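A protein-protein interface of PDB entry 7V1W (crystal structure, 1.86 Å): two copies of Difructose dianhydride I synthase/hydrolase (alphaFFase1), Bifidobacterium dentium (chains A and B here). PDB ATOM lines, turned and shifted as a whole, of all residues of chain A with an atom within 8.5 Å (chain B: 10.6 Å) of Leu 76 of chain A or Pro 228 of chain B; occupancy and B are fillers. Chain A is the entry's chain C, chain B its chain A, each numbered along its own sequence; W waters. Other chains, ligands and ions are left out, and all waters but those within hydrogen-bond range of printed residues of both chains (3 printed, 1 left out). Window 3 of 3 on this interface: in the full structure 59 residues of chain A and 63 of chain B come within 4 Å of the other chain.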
ATOM      1  N   LYS A  30      19.804  10.959  18.539  1.00  0.00           N
ATOM      2  CA  LYS A  30      19.234  12.132  17.820  1.00  0.00           C
ATOM      3  C   LYS A  30      17.761  11.817  17.510  1.00  0.00           C
ATOM      4  O   LYS A  30      17.206  10.961  18.188  1.00  0.00           O
ATOM      5  CB  LYS A  30      20.088  12.499  16.600  1.00  0.00           C
ATOM      6  CG  LYS A  30      21.534  12.857  16.942  1.00  0.00           C
ATOM      7  CD  LYS A  30      22.429  13.178  15.778  1.00  0.00           C
ATOM      8  CE  LYS A  30      23.819  13.595  16.233  1.00  0.00           C
ATOM      9  NZ  LYS A  30      24.518  14.318  15.153  1.00  0.00           N
ATOM     10  N   ASN A  31      17.137  12.492  16.549  1.00  0.00           N
ATOM     11  CA  ASN A  31      15.678  12.329  16.355  1.00  0.00           C
ATOM     12  C   ASN A  31      15.362  11.616  15.034  1.00  0.00           C
ATOM     13  O   ASN A  31      14.236  11.861  14.481  1.00  0.00           O
ATOM     14  CB  ASN A  31      14.955  13.663  16.479  1.00  0.00           C
ATOM     15  CG  ASN A  31      13.468  13.464  16.731  1.00  0.00           C
ATOM     16  OD1 ASN A  31      13.037  12.498  17.390  1.00  0.00           O
ATOM     17  ND2 ASN A  31      12.677  14.339  16.152  1.00  0.00           N
ATOM     18  N   GLN A  32      16.252  10.736  14.564  1.00  0.00           N
ATOM     19  CA  GLN A  32      15.922   9.797  13.465  1.00  0.00           C
ATOM     20  C   GLN A  32      15.615   8.415  14.057  1.00  0.00           C
ATOM     21  O   GLN A  32      16.401   7.467  13.828  1.00  0.00           O
ATOM     22  CB  GLN A  32      17.032   9.726  12.407  1.00  0.00           C
ATOM     23  CG  GLN A  32      17.231  11.007  11.609  1.00  0.00           C
ATOM     24  CD  GLN A  32      18.191  10.836  10.443  1.00  0.00           C
ATOM     25  OE1 GLN A  32      18.525   9.730  10.017  1.00  0.00           O
ATOM     26  NE2 GLN A  32      18.620  11.959   9.894  1.00  0.00           N
ATOM     27  N   LEU A  72      13.937  22.968  -1.329  1.00  0.00           N
ATOM     28  CA  LEU A  72      14.380  22.644   0.048  1.00  0.00           C
ATOM     29  C   LEU A  72      15.804  22.104  -0.067  1.00  0.00           C
ATOM     30  O   LEU A  72      15.991  21.145  -0.811  1.00  0.00           O
ATOM     31  CB  LEU A  72      13.442  21.615   0.705  1.00  0.00           C
ATOM     32  CG  LEU A  72      12.137  22.186   1.282  1.00  0.00           C
ATOM     33  CD1 LEU A  72      11.067  22.316   0.217  1.00  0.00           C
ATOM     34  CD2 LEU A  72      11.604  21.347   2.430  1.00  0.00           C
ATOM     35  N   ASP A  73      16.767  22.760   0.572  1.00  0.00           N
ATOM     36  CA  ASP A  73      18.176  22.279   0.660  1.00  0.00           C
ATOM     37  C   ASP A  73      18.155  20.805   1.056  1.00  0.00           C
ATOM     38  O   ASP A  73      17.721  20.490   2.165  1.00  0.00           O
ATOM     39  CB  ASP A  73      18.942  23.108   1.693  1.00  0.00           C
ATOM     40  CG  ASP A  73      20.395  22.684   1.891  1.00  0.00           C
ATOM     41  OD1 ASP A  73      20.627  21.577   2.392  1.00  0.00           O
ATOM     42  OD2 ASP A  73      21.276  23.492   1.578  1.00  0.00           O
ATOM     43  N   PRO A  74      18.576  19.859   0.179  1.00  0.00           N
ATOM     44  CA  PRO A  74      18.421  18.430   0.463  1.00  0.00           C
ATOM     45  C   PRO A  74      19.231  17.894   1.652  1.00  0.00           C
ATOM     46  O   PRO A  74      18.809  16.910   2.270  1.00  0.00           O
ATOM     47  CB  PRO A  74      18.845  17.712  -0.825  1.00  0.00           C
ATOM     48  CG  PRO A  74      19.576  18.754  -1.639  1.00  0.00           C
ATOM     49  CD  PRO A  74      19.109  20.112  -1.165  1.00  0.00           C
ATOM     50  N   GLU A  75      20.380  18.495   1.935  1.00  0.00           N
ATOM     51  CA  GLU A  75      21.263  18.045   3.037  1.00  0.00           C
ATOM     52  C   GLU A  75      20.579  18.418   4.368  1.00  0.00           C
ATOM     53  O   GLU A  75      20.379  17.531   5.201  1.00  0.00           O
ATOM     54  CB  GLU A  75      22.657  18.663   2.870  1.00  0.00           C
ATOM     55  CG  GLU A  75      23.459  18.095   1.697  1.00  0.00           C
ATOM     56  CD  GLU A  75      23.108  18.598   0.301  1.00  0.00           C
ATOM     57  OE1 GLU A  75      22.724  19.799   0.188  1.00  0.00           O
ATOM     58  OE2 GLU A  75      23.195  17.781  -0.671  1.00  0.00           O
ATOM     59  N   LEU A  76      20.192  19.680   4.550  1.00  0.00           N
ATOM     60  CA  LEU A  76      19.436  20.128   5.756  1.00  0.00           C
ATOM     61  C   LEU A  76      18.118  19.344   5.861  1.00  0.00           C
ATOM     62  O   LEU A  76      17.797  18.899   6.989  1.00  0.00           O
ATOM     63  CB  LEU A  76      19.210  21.639   5.705  1.00  0.00           C
ATOM     64  CG  LEU A  76      20.458  22.472   6.036  1.00  0.00           C
ATOM     65  CD1 LEU A  76      20.189  23.959   5.863  1.00  0.00           C
ATOM     66  CD2 LEU A  76      20.935  22.209   7.457  1.00  0.00           C
ATOM     67  N   ASN A  77      17.444  19.103   4.727  1.00  0.00           N
ATOM     68  CA  ASN A  77      16.076  18.523   4.694  1.00  0.00           C
ATOM     69  C   ASN A  77      16.149  17.136   5.318  1.00  0.00           C
ATOM     70  O   ASN A  77      15.180  16.738   5.988  1.00  0.00           O
ATOM     71  CB  ASN A  77      15.499  18.483   3.278  1.00  0.00           C
ATOM     72  CG  ASN A  77      13.993  18.345   3.160  1.00  0.00           C
ATOM     73  OD1 ASN A  77      13.488  18.352   2.042  1.00  0.00           O
ATOM     74  ND2 ASN A  77      13.266  18.171   4.254  1.00  0.00           N
ATOM     75  N   ALA A  78      17.289  16.453   5.162  1.00  0.00           N
ATOM     76  CA  ALA A  78      17.478  15.085   5.686  1.00  0.00           C
ATOM     77  C   ALA A  78      17.419  15.103   7.225  1.00  0.00           C
ATOM     78  O   ALA A  78      17.065  14.076   7.810  1.00  0.00           O
ATOM     79  CB  ALA A  78      18.772  14.503   5.177  1.00  0.00           C
ATOM     80  N   SER A  79      17.738  16.226   7.868  1.00  0.00           N
ATOM     81  CA  SER A  79      17.744  16.343   9.344  1.00  0.00           C
ATOM     82  C   SER A  79      16.436  16.952   9.864  1.00  0.00           C
ATOM     83  O   SER A  79      16.286  17.067  11.095  1.00  0.00           O
ATOM     84  CB  SER A  79      18.931  17.127   9.786  1.00  0.00           C
ATOM     85  OG  SER A  79      20.035  16.256   9.762  1.00  0.00           O
ATOM     86  N   ALA A  80      15.527  17.351   8.981  1.00  0.00           N
ATOM     87  CA  ALA A  80      14.207  17.865   9.398  1.00  0.00           C
ATOM     88  C   ALA A  80      13.289  16.668   9.666  1.00  0.00           C
ATOM     89  O   ALA A  80      13.774  15.529   9.899  1.00  0.00           O
ATOM     90  CB  ALA A  80      13.656  18.814   8.363  1.00  0.00           C
ATOM     91  N   ALA A  81      11.980  16.884   9.625  1.00  0.00           N
ATOM     92  CA  ALA A  81      11.026  15.774   9.723  1.00  0.00           C
ATOM     93  C   ALA A  81      11.373  14.782   8.613  1.00  0.00           C
ATOM     94  O   ALA A  81      11.884  15.164   7.568  1.00  0.00           O
ATOM     95  CB  ALA A  81       9.615  16.303   9.656  1.00  0.00           C
ATOM     96  N   MET A  84       8.164  14.577   3.933  1.00  0.00           N
ATOM     97  CA  MET A  84       7.704  15.896   3.481  1.00  0.00           C
ATOM     98  C   MET A  84       6.247  15.774   3.022  1.00  0.00           C
ATOM     99  O   MET A  84       5.976  15.654   1.804  1.00  0.00           O
ATOM    100  CB  MET A  84       8.655  16.479   2.438  1.00  0.00           C
ATOM    101  CG  MET A  84      10.046  16.760   3.030  1.00  0.00           C
ATOM    102  SD  MET A  84      10.020  18.073   4.256  1.00  0.00           S
ATOM    103  CE  MET A  84      10.220  17.132   5.773  1.00  0.00           C
ATOM    104  N   ARG A 416      21.595  14.384  -5.083  1.00  0.00           N
ATOM    105  CA  ARG A 416      21.773  14.926  -3.708  1.00  0.00           C
ATOM    106  C   ARG A 416      20.790  14.242  -2.742  1.00  0.00           C
ATOM    107  O   ARG A 416      21.211  13.965  -1.584  1.00  0.00           O
ATOM    108  CB  ARG A 416      21.686  16.446  -3.733  1.00  0.00           C
ATOM    109  CG  ARG A 416      22.856  17.055  -4.494  1.00  0.00           C
ATOM    110  CD  ARG A 416      22.650  18.503  -4.821  1.00  0.00           C
ATOM    111  NE  ARG A 416      22.651  19.272  -3.597  1.00  0.00           N
ATOM    112  CZ  ARG A 416      22.438  20.575  -3.533  1.00  0.00           C
ATOM    113  NH1 ARG A 416      22.219  21.266  -4.641  1.00  0.00           N
ATOM    114  NH2 ARG A 416      22.456  21.184  -2.361  1.00  0.00           N
ATOM    115  N   GLN A 420      21.492  11.239   0.465  1.00  0.00           N
ATOM    116  CA  GLN A 420      20.840  11.277   1.804  1.00  0.00           C
ATOM    117  C   GLN A 420      20.144   9.938   2.103  1.00  0.00           C
ATOM    118  O   GLN A 420      20.158   9.548   3.289  1.00  0.00           O
ATOM    119  CB  GLN A 420      19.899  12.474   1.922  1.00  0.00           C
ATOM    120  CG  GLN A 420      20.607  13.807   1.823  1.00  0.00           C
ATOM    121  CD  GLN A 420      21.804  13.897   2.729  1.00  0.00           C
ATOM    122  OE1 GLN A 420      21.779  13.452   3.874  1.00  0.00           O
ATOM    123  NE2 GLN A 420      22.855  14.500   2.206  1.00  0.00           N
ATOM    124  N   LYS A 424      21.165   7.191   5.342  1.00  0.00           N
ATOM    125  CA  LYS A 424      20.161   6.618   6.270  1.00  0.00           C
ATOM    126  C   LYS A 424      20.158   5.093   6.152  1.00  0.00           C
ATOM    127  O   LYS A 424      20.051   4.404   7.176  1.00  0.00           O
ATOM    128  CB  LYS A 424      18.803   7.267   5.996  1.00  0.00           C
ATOM    129  CG  LYS A 424      18.770   8.731   6.399  1.00  0.00           C
ATOM    130  CD  LYS A 424      17.558   9.508   5.894  1.00  0.00           C
ATOM    131  CE  LYS A 424      17.508  10.868   6.553  1.00  0.00           C
ATOM    132  NZ  LYS A 424      16.360  11.693   6.101  1.00  0.00           N
ATOM    133  N   TRP B 219      15.284  23.174  26.891  1.00  0.00           N
ATOM    134  CA  TRP B 219      16.492  23.904  26.416  1.00  0.00           C
ATOM    135  C   TRP B 219      16.156  24.772  25.196  1.00  0.00           C
ATOM    136  O   TRP B 219      16.951  25.686  24.919  1.00  0.00           O
ATOM    137  CB  TRP B 219      17.664  22.944  26.137  1.00  0.00           C
ATOM    138  CG  TRP B 219      17.452  21.956  25.033  1.00  0.00           C
ATOM    139  CD1 TRP B 219      17.103  20.645  25.154  1.00  0.00           C
ATOM    140  CD2 TRP B 219      17.609  22.185  23.622  1.00  0.00           C
ATOM    141  NE1 TRP B 219      17.009  20.054  23.917  1.00  0.00           N
ATOM    142  CE2 TRP B 219      17.307  20.977  22.962  1.00  0.00           C
ATOM    143  CE3 TRP B 219      17.976  23.293  22.850  1.00  0.00           C
ATOM    144  CZ2 TRP B 219      17.356  20.852  21.572  1.00  0.00           C
ATOM    145  CZ3 TRP B 219      18.054  23.165  21.481  1.00  0.00           C
ATOM    146  CH2 TRP B 219      17.747  21.962  20.855  1.00  0.00           C
ATOM    147  N   LEU B 223      12.805  27.373  19.597  1.00  0.00           N
ATOM    148  CA  LEU B 223      13.262  26.769  18.326  1.00  0.00           C
ATOM    149  C   LEU B 223      12.103  25.980  17.727  1.00  0.00           C
ATOM    150  O   LEU B 223      11.487  25.195  18.449  1.00  0.00           O
ATOM    151  CB  LEU B 223      14.457  25.838  18.555  1.00  0.00           C
ATOM    152  CG  LEU B 223      15.814  26.522  18.638  1.00  0.00           C
ATOM    153  CD1 LEU B 223      15.863  27.478  19.819  1.00  0.00           C
ATOM    154  CD2 LEU B 223      16.947  25.498  18.722  1.00  0.00           C
ATOM    155  N   GLN B 224      11.865  26.130  16.427  1.00  0.00           N
ATOM    156  CA  GLN B 224      10.902  25.272  15.691  1.00  0.00           C
ATOM    157  C   GLN B 224      11.227  23.793  15.935  1.00  0.00           C
ATOM    158  O   GLN B 224      12.361  23.319  15.629  1.00  0.00           O
ATOM    159  CB  GLN B 224      10.961  25.592  14.197  1.00  0.00           C
ATOM    160  CG  GLN B 224       9.929  24.846  13.387  1.00  0.00           C
ATOM    161  CD  GLN B 224       9.789  25.393  11.986  1.00  0.00           C
ATOM    162  OE1 GLN B 224      10.453  26.349  11.582  1.00  0.00           O
ATOM    163  NE2 GLN B 224       8.901  24.778  11.228  1.00  0.00           N
ATOM    164  N   VAL B 225      10.232  23.056  16.400  1.00  0.00           N
ATOM    165  CA  VAL B 225      10.238  21.565  16.416  1.00  0.00           C
ATOM    166  C   VAL B 225      10.632  21.038  15.036  1.00  0.00           C
ATOM    167  O   VAL B 225      10.070  21.519  14.003  1.00  0.00           O
ATOM    168  CB  VAL B 225       8.862  21.022  16.842  1.00  0.00           C
ATOM    169  CG1 VAL B 225       8.738  19.542  16.519  1.00  0.00           C
ATOM    170  CG2 VAL B 225       8.595  21.296  18.319  1.00  0.00           C
ATOM    171  N   ASN B 226      11.500  20.028  15.039  1.00  0.00           N
ATOM    172  CA  ASN B 226      11.911  19.227  13.870  1.00  0.00           C
ATOM    173  C   ASN B 226      12.791  20.074  12.938  1.00  0.00           C
ATOM    174  O   ASN B 226      13.061  19.623  11.822  1.00  0.00           O
ATOM    175  CB  ASN B 226      10.715  18.606  13.142  1.00  0.00           C
ATOM    176  CG  ASN B 226      10.196  17.371  13.840  1.00  0.00           C
ATOM    177  OD1 ASN B 226      10.971  16.639  14.434  1.00  0.00           O
ATOM    178  ND2 ASN B 226       8.896  17.135  13.800  1.00  0.00           N
ATOM    179  N   SER B 227      13.242  21.234  13.374  1.00  0.00           N
ATOM    180  CA  SER B 227      14.343  21.961  12.703  1.00  0.00           C
ATOM    181  C   SER B 227      15.607  21.096  12.779  1.00  0.00           C
ATOM    182  O   SER B 227      15.784  20.359  13.733  1.00  0.00           O
ATOM    183  CB  SER B 227      14.559  23.342  13.280  1.00  0.00           C
ATOM    184  OG  SER B 227      14.852  23.301  14.661  1.00  0.00           O
ATOM    185  N   PRO B 228      16.483  21.100  11.751  1.00  0.00           N
ATOM    186  CA  PRO B 228      17.701  20.289  11.772  1.00  0.00           C
ATOM    187  C   PRO B 228      18.559  20.532  13.017  1.00  0.00           C
ATOM    188  O   PRO B 228      19.190  19.583  13.452  1.00  0.00           O
ATOM    189  CB  PRO B 228      18.458  20.734  10.503  1.00  0.00           C
ATOM    190  CG  PRO B 228      17.375  21.239   9.574  1.00  0.00           C
ATOM    191  CD  PRO B 228      16.326  21.855  10.488  1.00  0.00           C
ATOM    192  N   GLU B 229      18.560  21.758  13.571  1.00  0.00           N
ATOM    193  CA  GLU B 229      19.357  22.101  14.786  1.00  0.00           C
ATOM    194  C   GLU B 229      18.813  21.319  15.991  1.00  0.00           C
ATOM    195  O   GLU B 229      19.629  20.738  16.764  1.00  0.00           O
ATOM    196  CB  GLU B 229      19.387  23.606  15.079  1.00  0.00           C
ATOM    197  CG  GLU B 229      20.073  24.437  13.995  1.00  0.00           C
ATOM    198  CD  GLU B 229      19.181  24.937  12.863  1.00  0.00           C
ATOM    199  OE1 GLU B 229      18.046  24.383  12.693  1.00  0.00           O
ATOM    200  OE2 GLU B 229      19.595  25.890  12.160  1.00  0.00           O
ATOM    201  N   VAL B 230      17.491  21.315  16.161  1.00  0.00           N
ATOM    202  CA  VAL B 230      16.828  20.570  17.268  1.00  0.00           C
ATOM    203  C   VAL B 230      17.133  19.096  17.081  1.00  0.00           C
ATOM    204  O   VAL B 230      17.532  18.454  18.056  1.00  0.00           O
ATOM    205  CB  VAL B 230      15.309  20.831  17.322  1.00  0.00           C
ATOM    206  CG1 VAL B 230      14.594  19.810  18.194  1.00  0.00           C
ATOM    207  CG2 VAL B 230      15.026  22.245  17.786  1.00  0.00           C
ATOM    208  N   ASN B 231      16.970  18.581  15.864  1.00  0.00           N
ATOM    209  CA  ASN B 231      16.949  17.125  15.612  1.00  0.00           C
ATOM    210  C   ASN B 231      18.349  16.543  15.734  1.00  0.00           C
ATOM    211  O   ASN B 231      18.416  15.324  15.815  1.00  0.00           O
ATOM    212  CB  ASN B 231      16.377  16.761  14.249  1.00  0.00           C
ATOM    213  CG  ASN B 231      14.855  16.756  14.238  1.00  0.00           C
ATOM    214  OD1 ASN B 231      14.214  16.678  15.278  1.00  0.00           O
ATOM    215  ND2 ASN B 231      14.276  16.812  13.060  1.00  0.00           N
ATOM    216  N   ASN B 232      19.399  17.358  15.748  1.00  0.00           N
ATOM    217  CA  ASN B 232      20.800  16.826  15.782  1.00  0.00           C
ATOM    218  C   ASN B 232      21.338  16.930  17.222  1.00  0.00           C
ATOM    219  O   ASN B 232      22.486  16.527  17.448  1.00  0.00           O
ATOM    220  CB  ASN B 232      21.666  17.443  14.666  1.00  0.00           C
ATOM    221  CG  ASN B 232      21.356  16.854  13.291  1.00  0.00           C
ATOM    222  OD1 ASN B 232      21.108  17.576  12.338  1.00  0.00           O
ATOM    223  ND2 ASN B 232      21.300  15.538  13.168  1.00  0.00           N
ATOM    224  N   VAL B 233      20.517  17.365  18.179  1.00  0.00           N
ATOM    225  CA  VAL B 233      20.914  17.382  19.614  1.00  0.00           C
ATOM    226  C   VAL B 233      20.750  15.962  20.146  1.00  0.00           C
ATOM    227  O   VAL B 233      19.735  15.304  19.823  1.00  0.00           O
ATOM    228  CB  VAL B 233      20.113  18.416  20.421  1.00  0.00           C
ATOM    229  CG1 VAL B 233      20.220  18.213  21.928  1.00  0.00           C
ATOM    230  CG2 VAL B 233      20.544  19.819  20.063  1.00  0.00           C
ATOM    231  N   THR B 234      21.730  15.471  20.898  1.00  0.00           N
ATOM    232  CA  THR B 234      21.723  14.067  21.393  1.00  0.00           C
ATOM    233  C   THR B 234      21.179  14.000  22.820  1.00  0.00           C
ATOM    234  O   THR B 234      21.343  14.988  23.560  1.00  0.00           O
ATOM    235  CB  THR B 234      23.112  13.408  21.353  1.00  0.00           C
ATOM    236  OG1 THR B 234      23.834  13.943  22.462  1.00  0.00           O
ATOM    237  CG2 THR B 234      23.812  13.640  20.035  1.00  0.00           C
ATOM    238  N   HIS B 346      11.819  16.181  21.504  1.00  0.00           N
ATOM    239  CA  HIS B 346      13.115  15.550  21.182  1.00  0.00           C
ATOM    240  C   HIS B 346      14.191  16.145  22.111  1.00  0.00           C
ATOM    241  O   HIS B 346      14.335  17.400  22.163  1.00  0.00           O
ATOM    242  CB  HIS B 346      13.505  15.742  19.717  1.00  0.00           C
ATOM    243  CG  HIS B 346      14.897  15.255  19.538  1.00  0.00           C
ATOM    244  ND1 HIS B 346      15.229  13.951  19.825  1.00  0.00           N
ATOM    245  CD2 HIS B 346      16.054  15.917  19.326  1.00  0.00           C
ATOM    246  CE1 HIS B 346      16.539  13.802  19.712  1.00  0.00           C
ATOM    247  NE2 HIS B 346      17.081  15.007  19.408  1.00  0.00           N
ATOM    248  N   ALA B 347      14.930  15.270  22.798  1.00  0.00           N
ATOM    249  CA  ALA B 347      16.024  15.653  23.715  1.00  0.00           C
ATOM    250  C   ALA B 347      15.561  16.717  24.721  1.00  0.00           C
ATOM    251  O   ALA B 347      16.365  17.557  25.133  1.00  0.00           O
ATOM    252  CB  ALA B 347      17.177  16.128  22.863  1.00  0.00           C
ATOM    253  N   GLN B 349      13.644  19.272  24.420  1.00  0.00           N
ATOM    254  CA  GLN B 349      13.642  20.600  23.778  1.00  0.00           C
ATOM    255  C   GLN B 349      12.556  21.474  24.404  1.00  0.00           C
ATOM    256  O   GLN B 349      12.821  22.677  24.675  1.00  0.00           O
ATOM    257  CB  GLN B 349      13.341  20.431  22.290  1.00  0.00           C
ATOM    258  CG  GLN B 349      13.207  21.746  21.546  1.00  0.00           C
ATOM    259  CD  GLN B 349      12.310  21.714  20.324  1.00  0.00           C
ATOM    260  OE1 GLN B 349      11.901  20.665  19.816  1.00  0.00           O
ATOM    261  NE2 GLN B 349      12.052  22.893  19.801  1.00  0.00           N
HETATM  262  O   HOH W   1      18.825  13.687  12.778  1.00  0.00           O
HETATM  263  O   HOH W   2      12.088  17.645  16.901  1.00  0.00           O
HETATM  264  O   HOH W   3      11.798  14.766  12.940  1.00  0.00           O
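The side-chain amide oxygen (OD1) of Asn 226 of chain B lies within hydrogen-bond range of the side-chain amide nitrogen (ND2) of Asn 31 of chain A (3.3 Å).
The side-chain amide oxygen (OD1) of Asn 231 of chain B is in hydrogen-bond range of the side-chain amide nitrogen (ND2) of Asn 31 of chain A (2.9 Å).
The backbone carbonyl oxygen (O) of Ser 79 of chain A is in hydrogen-bond range of the side-chain amide nitrogen (ND2) of Asn 231 of chain B (2.8 Å).
O of Ala 80 of chain A sits at hydrogen-bond distance from ND2 of Asn 231 of chain B (3.4 Å).
The side-chain hydroxyl (OG) of Ser 79 of chain A lies within hydrogen-bond range of the side-chain amide oxygen (OD1) of Asn 232 of chain B.
Of the printed residues of chain B, Lys 30 of chain A touches Asn 231, Asn 232, Val 233, Thr 234 and His 346.
Printed residues of chain B within 4 Å of Asn 31 of chain A: Asn 226, Asn 231 and His 346.
Asp 73 of chain A touches none of the printed residues of chain B.
Asn 77 of chain A touches none of the printed residues of chain B.
Printed residues of chain A within 4 Å of Asn 226 of chain B: Asn 31 (3.3 Å), Ala 80 (3.2 Å) and Ala 81 (3.7 Å).
No residue of chain A comes within 4 Å of Ser 227 of chain B.
Of chain A, only Leu 76 and Ser 79 come within 4 Å of Pro 228 of chain B.
Of the printed residues of chain A, Asn 231 of chain B touches Lys 30 (3.4 Å), Asn 31 (2.9 Å), Ser 79 (2.8 Å) and Ala 80 (3.4 Å).
The nearest residue of chain B that does not touch Leu 76 of chain A is Glu 229 of chain B (6.1 Å).
The nearest residue of chain A that does not touch Pro 228 of chain B is Ala 80 of chain A (4.3 Å).
Among the printed residues, pairs that only touch across the chains: Lys 30 of chain A with Asn 231 of chain B (3.4 Å), Lys 30 of chain A with Asn 232 of chain B (3.4 Å), Lys 30 of chain A with Val 233 of chain B (3.8 Å), Lys 30 of chain A with Thr 234 of chain B (3.8 Å), Lys 30 of chain A with His 346 of chain B (3.2 Å), Asn 31 of chain A with His 346 of chain B (3.4 Å), Leu 76 of chain A with Pro 228 of chain B (3.5 Å), Ser 79 of chain A with Pro 228 of chain B (3.6 Å), Ala 80 of chain A with Asn 226 of chain B (3.2 Å) and Ala 81 of chain A with Asn 226 of chain B (3.7 Å).
Water W3 lies within hydrogen-bond range of the side-chain amide oxygen of Asn 226 of chain B (2.5 Å), the side-chain amide nitrogen of Asn 231 of chain B (3.2 Å) and the side-chain amide nitrogen of Asn 31 of chain A (3.4 Å).
Water W2 lies within hydrogen-bond range of the side-chain amide oxygen of Asn 231 of chain B, the side-chain amide oxygen of Asn 226 of chain B and the side-chain amide nitrogen of Asn 31 of chain A.
Water W1 lies within hydrogen-bond range of the side-chain amide nitrogen of Asn 232 of chain B (3.1 Å), the side-chain amide nitrogen of Gln 32 of chain A (3.4 Å) and the backbone carbonyl oxygen of Asn 231 of chain B (3.5 Å).
The side-chain amide nitrogen of Asn 231 of chain B sits at hydrogen-bond distance from the backbone carbonyl oxygen of Asn 226 of chain B (3.3 Å).
The backbone carbonyl oxygen (O) of Pro 228 of chain B sits close to the side-chain amide oxygen (OD1) of Asn 232 of chain B (3.0 Å).
The backbone carbonyl oxygen (O) of Val 233 of chain B sits at hydrogen-bond distance from a ring nitrogen (NE2) of His 346 of chain B (2.7 Å).
The side-chain carboxylate (OD1) of Asp 73 of chain A lies within hydrogen-bond range of the backbone NH (N) of Leu 76 of chain A (2.9 Å).
Of the 17 printed residues of chain A, 6 touch a printed residue of chain B.
Hydrophobic or aromatic side chains of chain A that line the printed part of chain B: Ala 80.
Of the 16 printed residues of chain B, 7 touch a printed residue of chain A.
Printed residues of chain B that touch a printed residue of chain A: Asn 226, Pro 228, Asn 231, Asn 232, Val 233, Thr 234 and His 346.
No position is printed for both chains.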
